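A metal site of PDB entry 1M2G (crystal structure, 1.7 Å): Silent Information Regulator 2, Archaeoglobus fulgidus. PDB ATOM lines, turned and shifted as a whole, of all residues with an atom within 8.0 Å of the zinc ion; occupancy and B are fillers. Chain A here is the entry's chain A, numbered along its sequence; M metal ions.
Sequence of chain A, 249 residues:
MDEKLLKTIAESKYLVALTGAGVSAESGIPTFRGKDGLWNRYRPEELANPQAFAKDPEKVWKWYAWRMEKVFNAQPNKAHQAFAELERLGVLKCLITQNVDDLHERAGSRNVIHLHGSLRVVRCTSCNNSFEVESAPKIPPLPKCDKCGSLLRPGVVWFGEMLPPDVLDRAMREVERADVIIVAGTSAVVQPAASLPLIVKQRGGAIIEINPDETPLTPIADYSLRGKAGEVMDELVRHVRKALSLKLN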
ATOM      1  N   ARG A 123      13.582  -9.673  13.883  1.00  0.00           N
ATOM      2  CA  ARG A 123      12.728 -10.760  13.428  1.00  0.00           C
ATOM      3  C   ARG A 123      12.686 -10.867  11.923  1.00  0.00           C
ATOM      4  O   ARG A 123      13.039  -9.924  11.204  1.00  0.00           O
ATOM      5  CB  ARG A 123      11.305 -10.583  13.967  1.00  0.00           C
ATOM      6  CG  ARG A 123      10.564  -9.366  13.436  1.00  0.00           C
ATOM      7  CD  ARG A 123       9.220  -9.223  14.141  1.00  0.00           C
ATOM      8  NE  ARG A 123       8.420  -8.100  13.651  1.00  0.00           N
ATOM      9  CZ  ARG A 123       7.804  -8.069  12.474  1.00  0.00           C
ATOM     10  NH1 ARG A 123       7.870  -9.112  11.652  1.00  0.00           N
ATOM     11  NH2 ARG A 123       7.087  -7.007  12.128  1.00  0.00           N
ATOM     12  N   CYS A 124      12.258 -12.022  11.435  1.00  0.00           N
ATOM     13  CA  CYS A 124      12.154 -12.244  10.008  1.00  0.00           C
ATOM     14  C   CYS A 124      10.885 -11.621   9.460  1.00  0.00           C
ATOM     15  O   CYS A 124       9.846 -11.612  10.122  1.00  0.00           O
ATOM     16  CB  CYS A 124      12.151 -13.742   9.707  1.00  0.00           C
ATOM     17  SG  CYS A 124      11.916 -14.113   7.945  1.00  0.00           S
ATOM     18  N   THR A 125      10.981 -11.087   8.238  1.00  0.00           N
ATOM     19  CA  THR A 125       9.845 -10.453   7.598  1.00  0.00           C
ATOM     20  C   THR A 125       8.914 -11.509   7.010  1.00  0.00           C
ATOM     21  O   THR A 125       7.725 -11.238   6.762  1.00  0.00           O
ATOM     22  CB  THR A 125      10.308  -9.515   6.460  1.00  0.00           C
ATOM     23  OG1 THR A 125      11.081 -10.260   5.513  1.00  0.00           O
ATOM     24  CG2 THR A 125      11.164  -8.390   7.035  1.00  0.00           C
ATOM     25  N   SER A 126       9.450 -12.699   6.784  1.00  0.00           N
ATOM     26  CA  SER A 126       8.672 -13.804   6.236  1.00  0.00           C
ATOM     27  C   SER A 126       8.095 -14.682   7.335  1.00  0.00           C
ATOM     28  O   SER A 126       6.957 -14.493   7.759  1.00  0.00           O
ATOM     29  CB  SER A 126       9.557 -14.656   5.309  1.00  0.00           C
ATOM     30  OG  SER A 126      10.064 -13.882   4.234  1.00  0.00           O
ATOM     31  N   CYS A 127       8.885 -15.653   7.792  1.00  0.00           N
ATOM     32  CA  CYS A 127       8.435 -16.562   8.841  1.00  0.00           C
ATOM     33  C   CYS A 127       8.330 -15.847  10.180  1.00  0.00           C
ATOM     34  O   CYS A 127       9.084 -14.911  10.464  1.00  0.00           O
ATOM     35  CB  CYS A 127       9.405 -17.747   8.955  1.00  0.00           C
ATOM     36  SG  CYS A 127      11.065 -17.357   9.605  1.00  0.00           S
ATOM     37  N   ASN A 128       7.378 -16.276  10.999  1.00  0.00           N
ATOM     38  CA  ASN A 128       7.172 -15.680  12.312  1.00  0.00           C
ATOM     39  C   ASN A 128       8.249 -16.195  13.276  1.00  0.00           C
ATOM     40  O   ASN A 128       8.002 -17.132  14.041  1.00  0.00           O
ATOM     41  CB  ASN A 128       5.786 -16.027  12.850  1.00  0.00           C
ATOM     42  CG  ASN A 128       5.478 -15.358  14.186  1.00  0.00           C
ATOM     43  OD1 ASN A 128       5.500 -14.130  14.288  1.00  0.00           O
ATOM     44  ND2 ASN A 128       5.201 -16.158  15.202  1.00  0.00           N
ATOM     45  N   ASN A 129       9.423 -15.584  13.217  1.00  0.00           N
ATOM     46  CA  ASN A 129      10.545 -15.978  14.066  1.00  0.00           C
ATOM     47  C   ASN A 129      11.389 -14.766  14.457  1.00  0.00           C
ATOM     48  O   ASN A 129      11.721 -13.927  13.624  1.00  0.00           O
ATOM     49  CB  ASN A 129      11.419 -16.994  13.331  1.00  0.00           C
ATOM     50  CG  ASN A 129      12.619 -17.415  14.142  1.00  0.00           C
ATOM     51  OD1 ASN A 129      12.482 -17.944  15.250  1.00  0.00           O
ATOM     52  ND2 ASN A 129      13.813 -17.203  13.593  1.00  0.00           N
ATOM     53  N   SER A 130      11.742 -14.690  15.736  1.00  0.00           N
ATOM     54  CA  SER A 130      12.545 -13.580  16.237  1.00  0.00           C
ATOM     55  C   SER A 130      13.538 -14.033  17.295  1.00  0.00           C
ATOM     56  O   SER A 130      13.457 -15.150  17.811  1.00  0.00           O
ATOM     57  CB  SER A 130      11.642 -12.506  16.823  1.00  0.00           C
ATOM     58  OG  SER A 130      10.999 -12.972  17.995  1.00  0.00           O
ATOM     59  N   LYS A 144      20.178 -11.374   7.392  1.00  0.00           N
ATOM     60  CA  LYS A 144      19.302 -12.357   6.769  1.00  0.00           C
ATOM     61  C   LYS A 144      18.819 -13.437   7.727  1.00  0.00           C
ATOM     62  O   LYS A 144      19.517 -13.790   8.679  1.00  0.00           O
ATOM     63  CB  LYS A 144      20.008 -12.984   5.573  1.00  0.00           C
ATOM     64  CG  LYS A 144      20.577 -11.971   4.600  1.00  0.00           C
ATOM     65  CD  LYS A 144      21.241 -12.619   3.405  1.00  0.00           C
ATOM     66  CE  LYS A 144      21.930 -11.592   2.526  1.00  0.00           C
ATOM     67  NZ  LYS A 144      20.997 -10.525   2.066  1.00  0.00           N
ATOM     68  N   CYS A 145      17.622 -13.944   7.471  1.00  0.00           N
ATOM     69  CA  CYS A 145      17.027 -14.986   8.290  1.00  0.00           C
ATOM     70  C   CYS A 145      17.581 -16.350   7.915  1.00  0.00           C
ATOM     71  O   CYS A 145      17.497 -16.777   6.769  1.00  0.00           O
ATOM     72  CB  CYS A 145      15.502 -14.985   8.120  1.00  0.00           C
ATOM     73  SG  CYS A 145      14.667 -16.362   8.973  1.00  0.00           S
ATOM     74  N   ASP A 146      18.140 -17.038   8.916  1.00  0.00           N
ATOM     75  CA  ASP A 146      18.713 -18.362   8.695  1.00  0.00           C
ATOM     76  C   ASP A 146      17.660 -19.450   8.864  1.00  0.00           C
ATOM     77  O   ASP A 146      17.991 -20.593   9.192  1.00  0.00           O
ATOM     78  CB  ASP A 146      19.869 -18.599   9.669  1.00  0.00           C
ATOM     79  CG  ASP A 146      19.459 -18.448  11.121  1.00  0.00           C
ATOM     80  OD1 ASP A 146      18.602 -19.235  11.577  1.00  0.00           O
ATOM     81  OD2 ASP A 146      19.988 -17.547  11.808  1.00  0.00           O
ATOM     82  N   LYS A 147      16.406 -19.100   8.619  1.00  0.00           N
ATOM     83  CA  LYS A 147      15.310 -20.060   8.752  1.00  0.00           C
ATOM     84  C   LYS A 147      14.480 -20.210   7.479  1.00  0.00           C
ATOM     85  O   LYS A 147      13.616 -21.083   7.403  1.00  0.00           O
ATOM     86  CB  LYS A 147      14.388 -19.673   9.914  1.00  0.00           C
ATOM     87  CG  LYS A 147      15.031 -19.825  11.281  1.00  0.00           C
ATOM     88  CD  LYS A 147      15.432 -21.264  11.535  1.00  0.00           C
ATOM     89  CE  LYS A 147      16.107 -21.437  12.888  1.00  0.00           C
ATOM     90  NZ  LYS A 147      16.540 -22.839  13.109  1.00  0.00           N
ATOM     91  N   CYS A 148      14.742 -19.372   6.478  1.00  0.00           N
ATOM     92  CA  CYS A 148      13.990 -19.439   5.235  1.00  0.00           C
ATOM     93  C   CYS A 148      14.617 -18.607   4.126  1.00  0.00           C
ATOM     94  O   CYS A 148      14.040 -18.460   3.042  1.00  0.00           O
ATOM     95  CB  CYS A 148      12.548 -18.980   5.461  1.00  0.00           C
ATOM     96  SG  CYS A 148      12.424 -17.267   6.065  1.00  0.00           S
ATOM     97  N   GLY A 149      15.797 -18.052   4.386  1.00  0.00           N
ATOM     98  CA  GLY A 149      16.467 -17.239   3.380  1.00  0.00           C
ATOM     99  C   GLY A 149      15.675 -16.014   2.977  1.00  0.00           C
ATOM    100  O   GLY A 149      15.210 -15.905   1.839  1.00  0.00           O
ATOM    101  N   SER A 150      15.533 -15.084   3.918  1.00  0.00           N
ATOM    102  CA  SER A 150      14.807 -13.837   3.683  1.00  0.00           C
ATOM    103  C   SER A 150      15.458 -12.766   4.550  1.00  0.00           C
ATOM    104  O   SER A 150      16.482 -13.016   5.187  1.00  0.00           O
ATOM    105  CB  SER A 150      13.335 -14.001   4.055  1.00  0.00           C
ATOM    106  OG  SER A 150      13.196 -14.492   5.375  1.00  0.00           O
ATOM    107  N   LEU A 151      14.878 -11.568   4.582  1.00  0.00           N
ATOM    108  CA  LEU A 151      15.452 -10.485   5.375  1.00  0.00           C
ATOM    109  C   LEU A 151      14.929 -10.387   6.801  1.00  0.00           C
ATOM    110  O   LEU A 151      13.769 -10.699   7.082  1.00  0.00           O
ATOM    111  CB  LEU A 151      15.214  -9.141   4.685  1.00  0.00           C
ATOM    112  CG  LEU A 151      15.871  -8.909   3.326  1.00  0.00           C
ATOM    113  CD1 LEU A 151      15.527  -7.507   2.831  1.00  0.00           C
ATOM    114  CD2 LEU A 151      17.378  -9.078   3.433  1.00  0.00           C
ATOM    115  N   LEU A 152      15.814  -9.965   7.702  1.00  0.00           N
ATOM    116  CA  LEU A 152      15.456  -9.755   9.098  1.00  0.00           C
ATOM    117  C   LEU A 152      15.173  -8.265   9.197  1.00  0.00           C
ATOM    118  O   LEU A 152      15.645  -7.491   8.366  1.00  0.00           O
ATOM    119  CB  LEU A 152      16.616 -10.119  10.027  1.00  0.00           C
ATOM    120  CG  LEU A 152      16.896 -11.603  10.280  1.00  0.00           C
ATOM    121  CD1 LEU A 152      18.216 -11.752  11.024  1.00  0.00           C
ATOM    122  CD2 LEU A 152      15.749 -12.200  11.081  1.00  0.00           C
HETATM  123 ZN    ZN M   1      12.528 -16.287   8.152  1.00  0.00          ZN
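The zinc ion is bound by SG of Cys 124 (2.3 Å), SG of Cys 145 (2.3 Å), SG of Cys 148 (2.3 Å) and SG of Cys 127 (2.3 Å).
OG of Ser 150 touches the zinc ion (3.4 Å). Within 4 Å of the zinc ion: Cys 124, Cys 127, Cys 145, Cys 148 and Ser 150.
The side-chain hydroxyl (OG) of Ser 150 lies close to the side-chain sulfur (SG) of Cys 124, at 2.9 Å. The backbone NH of Ser 126 sits close to the side-chain sulfur of Cys 124 (3.1 Å). N of Cys 124 is in hydrogen-bond range of O of Asn 129, 3.0 Å away. The backbone carbonyl oxygen of Ser 150 sits at hydrogen-bond distance from the backbone NH of Cys 145, at 2.7 Å. The side-chain sulfur (SG) of Cys 145 lies close to the backbone NH (N) of Lys 147 (3.3 Å). SG of Cys 148 lies close to OG of Ser 150. The side-chain hydroxyl (OG) of Ser 150 sits close to the side-chain hydroxyl (OG) of Ser 126.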
